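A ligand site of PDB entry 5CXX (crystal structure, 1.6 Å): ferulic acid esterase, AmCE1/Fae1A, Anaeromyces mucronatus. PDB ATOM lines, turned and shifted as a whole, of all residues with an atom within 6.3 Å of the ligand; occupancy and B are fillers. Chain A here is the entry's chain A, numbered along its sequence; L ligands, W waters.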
ATOM      1  N   HIS A  63      15.649  -7.147 -28.467  1.00  0.00           N
ATOM      2  CA  HIS A  63      16.059  -6.072 -27.588  1.00  0.00           C
ATOM      3  C   HIS A  63      15.831  -4.682 -28.128  1.00  0.00           C
ATOM      4  O   HIS A  63      15.425  -4.476 -29.276  1.00  0.00           O
ATOM      5  CB  HIS A  63      17.561  -6.268 -27.300  1.00  0.00           C
ATOM      6  CG  HIS A  63      18.445  -6.131 -28.533  1.00  0.00           C
ATOM      7  ND1 HIS A  63      18.730  -4.906 -29.109  1.00  0.00           N
ATOM      8  CD2 HIS A  63      19.099  -7.066 -29.269  1.00  0.00           C
ATOM      9  CE1 HIS A  63      19.539  -5.086 -30.154  1.00  0.00           C
ATOM     10  NE2 HIS A  63      19.762  -6.387 -30.281  1.00  0.00           N
ATOM     11  N   GLY A  64      16.122  -3.697 -27.280  1.00  0.00           N
ATOM     12  CA  GLY A  64      15.945  -2.303 -27.637  1.00  0.00           C
ATOM     13  C   GLY A  64      17.180  -1.612 -28.215  1.00  0.00           C
ATOM     14  O   GLY A  64      18.219  -2.245 -28.546  1.00  0.00           O
ATOM     15  N   LEU A  65      17.051  -0.302 -28.348  1.00  0.00           N
ATOM     16  CA  LEU A  65      18.109   0.464 -28.968  1.00  0.00           C
ATOM     17  C   LEU A  65      19.383   0.335 -28.127  1.00  0.00           C
ATOM     18  O   LEU A  65      19.338   0.298 -26.890  1.00  0.00           O
ATOM     19  CB  LEU A  65      17.696   1.983 -29.016  1.00  0.00           C
ATOM     20  CG  LEU A  65      18.233   2.835 -30.135  1.00  0.00           C
ATOM     21  CD1 LEU A  65      17.701   2.326 -31.486  1.00  0.00           C
ATOM     22  CD2 LEU A  65      17.881   4.304 -29.837  1.00  0.00           C
ATOM     23  N   MET A  66      20.505   0.302 -28.792  1.00  0.00           N
ATOM     24  CA  MET A  66      21.811   0.328 -28.086  1.00  0.00           C
ATOM     25  C   MET A  66      22.080  -0.928 -27.216  1.00  0.00           C
ATOM     26  O   MET A  66      22.977  -0.945 -26.377  1.00  0.00           O
ATOM     27  CB  MET A  66      22.001   1.596 -27.230  1.00  0.00           C
ATOM     28  CG  MET A  66      21.494   2.866 -28.024  1.00  0.00           C
ATOM     29  SD  MET A  66      22.048   4.243 -27.175  1.00  0.00           S
ATOM     30  CE  MET A  66      20.951   5.500 -27.976  1.00  0.00           C
ATOM     31  N   PHE A 114      20.624   8.224 -30.779  1.00  0.00           N
ATOM     32  CA  PHE A 114      19.269   8.571 -31.242  1.00  0.00           C
ATOM     33  C   PHE A 114      19.388   9.358 -32.555  1.00  0.00           C
ATOM     34  O   PHE A 114      19.324  10.605 -32.586  1.00  0.00           O
ATOM     35  CB  PHE A 114      18.581   9.397 -30.161  1.00  0.00           C
ATOM     36  CG  PHE A 114      18.358   8.620 -28.868  1.00  0.00           C
ATOM     37  CD1 PHE A 114      17.321   7.696 -28.757  1.00  0.00           C
ATOM     38  CD2 PHE A 114      19.201   8.858 -27.753  1.00  0.00           C
ATOM     39  CE1 PHE A 114      17.106   6.992 -27.564  1.00  0.00           C
ATOM     40  CE2 PHE A 114      18.976   8.149 -26.551  1.00  0.00           C
ATOM     41  CZ  PHE A 114      17.952   7.243 -26.461  1.00  0.00           C
ATOM     42  N   TYR A 119      18.769   4.066 -36.590  1.00  0.00           N
ATOM     43  CA  TYR A 119      17.519   3.325 -36.655  1.00  0.00           C
ATOM     44  C   TYR A 119      17.376   2.448 -37.877  1.00  0.00           C
ATOM     45  O   TYR A 119      16.684   1.405 -37.779  1.00  0.00           O
ATOM     46  CB  TYR A 119      16.349   4.329 -36.630  1.00  0.00           C
ATOM     47  CG  TYR A 119      16.355   5.331 -35.500  1.00  0.00           C
ATOM     48  CD1 TYR A 119      16.958   5.083 -34.259  1.00  0.00           C
ATOM     49  CD2 TYR A 119      15.673   6.547 -35.654  1.00  0.00           C
ATOM     50  CE1 TYR A 119      16.957   6.030 -33.247  1.00  0.00           C
ATOM     51  CE2 TYR A 119      15.627   7.464 -34.606  1.00  0.00           C
ATOM     52  CZ  TYR A 119      16.264   7.200 -33.428  1.00  0.00           C
ATOM     53  OH  TYR A 119      16.253   8.158 -32.440  1.00  0.00           O
ATOM     54  N   PHE A 155      11.215  -5.298 -26.858  1.00  0.00           N
ATOM     55  CA  PHE A 155      11.160  -4.150 -25.983  1.00  0.00           C
ATOM     56  C   PHE A 155      11.635  -2.910 -26.720  1.00  0.00           C
ATOM     57  O   PHE A 155      12.670  -2.952 -27.380  1.00  0.00           O
ATOM     58  CB  PHE A 155      12.075  -4.406 -24.794  1.00  0.00           C
ATOM     59  CG  PHE A 155      12.270  -3.205 -23.899  1.00  0.00           C
ATOM     60  CD1 PHE A 155      11.204  -2.646 -23.216  1.00  0.00           C
ATOM     61  CD2 PHE A 155      13.588  -2.713 -23.668  1.00  0.00           C
ATOM     62  CE1 PHE A 155      11.398  -1.574 -22.335  1.00  0.00           C
ATOM     63  CE2 PHE A 155      13.779  -1.611 -22.771  1.00  0.00           C
ATOM     64  CZ  PHE A 155      12.693  -1.056 -22.132  1.00  0.00           C
ATOM     65  N   SER A 156      10.851  -1.829 -26.590  1.00  0.00           N
ATOM     66  CA  SER A 156      11.241  -0.466 -27.020  1.00  0.00           C
ATOM     67  C   SER A 156      11.563  -0.498 -28.503  1.00  0.00           C
ATOM     68  O   SER A 156      10.635  -0.746 -29.295  1.00  0.00           O
ATOM     69  CB  SER A 156      12.353   0.093 -26.160  1.00  0.00           C
ATOM     70  OG  SER A 156      12.319   1.492 -26.286  1.00  0.00           O
ATOM     71  N   MET A 157      12.794  -0.183 -28.934  1.00  0.00           N
ATOM     72  CA  MET A 157      12.991  -0.262 -30.373  1.00  0.00           C
ATOM     73  C   MET A 157      12.667  -1.661 -30.930  1.00  0.00           C
ATOM     74  O   MET A 157      12.221  -1.794 -32.075  1.00  0.00           O
ATOM     75  CB  MET A 157      14.489   0.084 -30.726  1.00  0.00           C
ATOM     76  CG  MET A 157      14.665   0.342 -32.230  1.00  0.00           C
ATOM     77  SD  MET A 157      13.931   1.960 -32.690  1.00  0.00           S
ATOM     78  CE  MET A 157      14.427   2.054 -34.421  1.00  0.00           C
ATOM     79  N   GLY A 158      12.922  -2.704 -30.140  1.00  0.00           N
ATOM     80  CA  GLY A 158      12.634  -4.092 -30.579  1.00  0.00           C
ATOM     81  C   GLY A 158      11.119  -4.327 -30.643  1.00  0.00           C
ATOM     82  O   GLY A 158      10.674  -5.182 -31.423  1.00  0.00           O
ATOM     83  N   ARG A 160       8.924  -1.731 -31.447  1.00  0.00           N
ATOM     84  CA  ARG A 160       8.613  -1.073 -32.714  1.00  0.00           C
ATOM     85  C   ARG A 160       8.882  -2.015 -33.881  1.00  0.00           C
ATOM     86  O   ARG A 160       8.046  -2.160 -34.800  1.00  0.00           O
ATOM     87  CB  ARG A 160       9.450   0.226 -32.816  1.00  0.00           C
ATOM     88  CG  ARG A 160       9.819   0.536 -34.269  1.00  0.00           C
ATOM     89  CD  ARG A 160      10.434   1.972 -34.389  1.00  0.00           C
ATOM     90  NE  ARG A 160      11.192   2.009 -35.624  1.00  0.00           N
ATOM     91  CZ  ARG A 160      11.632   3.166 -36.153  1.00  0.00           C
ATOM     92  NH1 ARG A 160      11.342   4.339 -35.551  1.00  0.00           N
ATOM     93  NH2 ARG A 160      12.371   3.140 -37.260  1.00  0.00           N
ATOM     94  N   ALA A 182       8.896   1.932 -29.346  1.00  0.00           N
ATOM     95  CA  ALA A 182       9.490   3.229 -29.647  1.00  0.00           C
ATOM     96  C   ALA A 182       8.688   4.014 -30.704  1.00  0.00           C
ATOM     97  O   ALA A 182       7.986   3.395 -31.531  1.00  0.00           O
ATOM     98  CB  ALA A 182      10.964   2.967 -30.156  1.00  0.00           C
ATOM     99  N   PRO A 183       8.873   5.332 -30.748  1.00  0.00           N
ATOM    100  CA  PRO A 183       8.260   6.135 -31.812  1.00  0.00           C
ATOM    101  C   PRO A 183       8.773   5.785 -33.179  1.00  0.00           C
ATOM    102  O   PRO A 183       9.883   5.239 -33.343  1.00  0.00           O
ATOM    103  CB  PRO A 183       8.673   7.575 -31.489  1.00  0.00           C
ATOM    104  CG  PRO A 183       9.943   7.432 -30.585  1.00  0.00           C
ATOM    105  CD  PRO A 183       9.706   6.155 -29.819  1.00  0.00           C
ATOM    106  N   GLY A 184       7.971   6.126 -34.193  1.00  0.00           N
ATOM    107  CA  GLY A 184       8.397   6.134 -35.579  1.00  0.00           C
ATOM    108  C   GLY A 184       7.912   4.993 -36.455  1.00  0.00           C
ATOM    109  O   GLY A 184       8.301   4.938 -37.656  1.00  0.00           O
ATOM    110  N   ASP A 190       9.552  13.663 -31.428  1.00  0.00           N
ATOM    111  CA  ASP A 190       9.870  13.572 -29.993  1.00  0.00           C
ATOM    112  C   ASP A 190      11.129  14.323 -29.641  1.00  0.00           C
ATOM    113  O   ASP A 190      11.789  14.933 -30.502  1.00  0.00           O
ATOM    114  CB  ASP A 190       9.955  12.119 -29.503  1.00  0.00           C
ATOM    115  CG  ASP A 190      11.291  11.434 -29.853  1.00  0.00           C
ATOM    116  OD1 ASP A 190      12.060  11.912 -30.698  1.00  0.00           O
ATOM    117  OD2 ASP A 190      11.505  10.363 -29.262  1.00  0.00           O
ATOM    118  N   SER A 191      11.469  14.293 -28.353  1.00  0.00           N
ATOM    119  CA  SER A 191      12.582  15.087 -27.869  1.00  0.00           C
ATOM    120  C   SER A 191      13.949  14.419 -28.113  1.00  0.00           C
ATOM    121  O   SER A 191      14.965  15.071 -28.051  1.00  0.00           O
ATOM    122  CB  SER A 191      12.420  15.328 -26.361  1.00  0.00           C
ATOM    123  OG  SER A 191      12.427  14.048 -25.702  1.00  0.00           O
ATOM    124  N   PHE A 192      13.973  13.118 -28.330  1.00  0.00           N
ATOM    125  CA  PHE A 192      15.237  12.395 -28.535  1.00  0.00           C
ATOM    126  C   PHE A 192      15.787  12.595 -29.931  1.00  0.00           C
ATOM    127  O   PHE A 192      17.017  12.786 -30.080  1.00  0.00           O
ATOM    128  CB  PHE A 192      14.984  10.898 -28.278  1.00  0.00           C
ATOM    129  CG  PHE A 192      14.760  10.580 -26.836  1.00  0.00           C
ATOM    130  CD1 PHE A 192      13.489  10.621 -26.293  1.00  0.00           C
ATOM    131  CD2 PHE A 192      15.833  10.244 -26.028  1.00  0.00           C
ATOM    132  CE1 PHE A 192      13.272  10.362 -24.949  1.00  0.00           C
ATOM    133  CE2 PHE A 192      15.630   9.985 -24.682  1.00  0.00           C
ATOM    134  CZ  PHE A 192      14.325  10.063 -24.140  1.00  0.00           C
ATOM    135  N   SER A 193      14.940  12.487 -30.971  1.00  0.00           N
ATOM    136  CA  SER A 193      15.506  12.737 -32.298  1.00  0.00           C
ATOM    137  C   SER A 193      14.604  13.547 -33.244  1.00  0.00           C
ATOM    138  O   SER A 193      14.867  13.613 -34.443  1.00  0.00           O
ATOM    139  CB  SER A 193      15.921  11.440 -33.004  1.00  0.00           C
ATOM    140  OG  SER A 193      14.818  10.574 -33.098  1.00  0.00           O
ATOM    141  N   GLY A 194      13.640  14.257 -32.693  1.00  0.00           N
ATOM    142  CA  GLY A 194      12.973  15.221 -33.562  1.00  0.00           C
ATOM    143  C   GLY A 194      11.960  14.513 -34.437  1.00  0.00           C
ATOM    144  O   GLY A 194      11.202  13.657 -33.964  1.00  0.00           O
ATOM    145  N   HIS A 196      10.167  12.053 -36.876  1.00  0.00           N
ATOM    146  CA  HIS A 196      10.230  10.687 -37.344  1.00  0.00           C
ATOM    147  C   HIS A 196       9.334  10.603 -38.569  1.00  0.00           C
ATOM    148  O   HIS A 196       8.140  10.830 -38.434  1.00  0.00           O
ATOM    149  CB  HIS A 196       9.730   9.726 -36.286  1.00  0.00           C
ATOM    150  CG  HIS A 196      10.581   9.684 -35.064  1.00  0.00           C
ATOM    151  ND1 HIS A 196      10.753  10.767 -34.220  1.00  0.00           N
ATOM    152  CD2 HIS A 196      11.327   8.678 -34.534  1.00  0.00           C
ATOM    153  CE1 HIS A 196      11.558  10.424 -33.216  1.00  0.00           C
ATOM    154  NE2 HIS A 196      11.912   9.161 -33.385  1.00  0.00           N
ATOM    155  N   VAL A 224      11.138   7.327 -21.797  1.00  0.00           N
ATOM    156  CA  VAL A 224      11.905   7.149 -23.034  1.00  0.00           C
ATOM    157  C   VAL A 224      10.956   7.120 -24.246  1.00  0.00           C
ATOM    158  O   VAL A 224      11.255   7.805 -25.236  1.00  0.00           O
ATOM    159  CB  VAL A 224      12.724   5.871 -23.000  1.00  0.00           C
ATOM    160  CG1 VAL A 224      13.459   5.545 -24.359  1.00  0.00           C
ATOM    161  CG2 VAL A 224      13.752   5.981 -21.855  1.00  0.00           C
ATOM    162  N   VAL A 225       9.855   6.354 -24.146  1.00  0.00           N
ATOM    163  CA  VAL A 225       8.954   6.314 -25.306  1.00  0.00           C
ATOM    164  C   VAL A 225       7.603   7.006 -25.032  1.00  0.00           C
ATOM    165  O   VAL A 225       6.807   7.096 -25.932  1.00  0.00           O
ATOM    166  CB  VAL A 225       8.688   4.847 -25.803  1.00  0.00           C
ATOM    167  CG1 VAL A 225      10.060   4.156 -26.187  1.00  0.00           C
ATOM    168  CG2 VAL A 225       7.915   3.962 -24.776  1.00  0.00           C
ATOM    169  N   HIS A 253      10.570   2.913 -18.210  1.00  0.00           N
ATOM    170  CA  HIS A 253      11.216   2.115 -19.252  1.00  0.00           C
ATOM    171  C   HIS A 253      12.050   1.027 -18.520  1.00  0.00           C
ATOM    172  O   HIS A 253      13.264   1.178 -18.329  1.00  0.00           O
ATOM    173  CB  HIS A 253      12.093   3.009 -20.147  1.00  0.00           C
ATOM    174  CG  HIS A 253      12.113   2.623 -21.614  1.00  0.00           C
ATOM    175  ND1 HIS A 253      10.965   2.448 -22.374  1.00  0.00           N
ATOM    176  CD2 HIS A 253      13.159   2.377 -22.441  1.00  0.00           C
ATOM    177  CE1 HIS A 253      11.301   2.129 -23.604  1.00  0.00           C
ATOM    178  NE2 HIS A 253      12.638   2.081 -23.672  1.00  0.00           N
HETATM  179  C1  LIG L   1      13.361   7.631 -30.084  1.00  0.00           C
HETATM  180  C2  LIG L   1      13.414   7.459 -28.670  1.00  0.00           C
HETATM  181  C3  LIG L   1      13.680   6.235 -28.152  1.00  0.00           C
HETATM  182  C4  LIG L   1      13.493   6.500 -30.906  1.00  0.00           C
HETATM  183  C5  LIG L   1      13.790   5.258 -30.401  1.00  0.00           C
HETATM  184  C6  LIG L   1      13.865   5.109 -29.026  1.00  0.00           C
HETATM  185  C7  LIG L   1      13.310   5.589 -33.013  1.00  0.00           C
HETATM  186  C8  LIG L   1      14.211   3.769 -28.490  1.00  0.00           C
HETATM  187  C9  LIG L   1      14.646   3.538 -27.231  1.00  0.00           C
HETATM  188  C10 LIG L   1      14.955   2.100 -26.823  1.00  0.00           C
HETATM  189  O1  LIG L   1      14.844   1.125 -27.628  1.00  0.00           O
HETATM  190  O2  LIG L   1      15.364   1.889 -25.654  1.00  0.00           O
HETATM  191  O3  LIG L   1      13.094   8.807 -30.719  1.00  0.00           O
HETATM  192  O4  LIG L   1      13.376   6.778 -32.233  1.00  0.00           O
HETATM  193  O   HOH W   1      17.019  -0.256 -25.079  1.00  0.00           O
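The backbone carbonyl oxygen (O) of Pro 183 lies within hydrogen-bond range of the guanidinium group (NH1) of Arg 160 (2.8 Å).
OD1 of Asp 190 lies within hydrogen-bond range of N of Ser 193 (2.9 Å).
The side-chain carboxylate (OD1) of Asp 190 sits at hydrogen-bond distance from the backbone NH (N) of Gly 194 (3.5 Å).
OD1 of Asp 190 sits at hydrogen-bond distance from N of Phe 192.
The side-chain hydroxyl (OH) of Tyr 119 sits at hydrogen-bond distance from the side-chain hydroxyl (OG) of Ser 193 (2.9 Å).
The backbone carbonyl oxygen of Gly 194 lies within hydrogen-bond range of a ring nitrogen (ND1) of His 196.
The backbone carbonyl oxygen (O) of Ser 156 is in hydrogen-bond range of the backbone NH (N) of Ala 182, at 3.2 Å.
A ring nitrogen (NE2) of His 253 is in hydrogen-bond range of the side-chain hydroxyl (OG) of Ser 156 (2.7 Å).
The side-chain carboxylate (OD2) of Asp 190 lies within hydrogen-bond range of an oxygen (O3) of the ligand.
An oxygen (O3) of the ligand is in hydrogen-bond range of a ring nitrogen (NE2) of His 196.
NE2 of His 253 sits at hydrogen-bond distance from O2 of the ligand (3.4 Å).
N of Leu 65 lies within hydrogen-bond range of O1 of the ligand (2.7 Å).
The backbone NH (N) of Met 157 lies within hydrogen-bond range of an oxygen (O1) of the ligand (2.8 Å).
OG of Ser 156 sits close to O1 of the ligand (2.9 Å).
The side-chain hydroxyl (OH) of Tyr 119 lies close to an oxygen (O4) of the ligand (3.2 Å).
OG of Ser 193 sits at hydrogen-bond distance from O3 of the ligand, at 3.4 Å.
Gly 64 touches the ligand.
CE1 of Phe 114 touches C3 of the ligand, at 3.6 Å.
Arg 160 touches the ligand (NH1 to C7, 3.4 Å).
Ala 182 touches the ligand (CB to C5, 3.6 Å).
Pro 183 touches the ligand.
Phe 192 touches the ligand (CB to O3, 3.7 Å).
CG1 of Val 224 touches C9 of the ligand (3.7 Å).
Hydrophobic or aromatic side chains within 4 Å of the ligand: Leu 65, Phe 114, Tyr 119, Met 157, Ala 182, Pro 183, Phe 192, His 196, Val 224 and His 253.
15 residues have an atom within 4 Å of the ligand: Gly 64, Leu 65, Phe 114, Tyr 119, Ser 156, Met 157, Arg 160, Ala 182, Pro 183, Asp 190, Phe 192, Ser 193, His 196, Val 224 and His 253.
Along chain A the residues within 4 Å of the ligand span positions 64 to 253.
Water W1 bridges O2 of the ligand and O of Leu 65.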
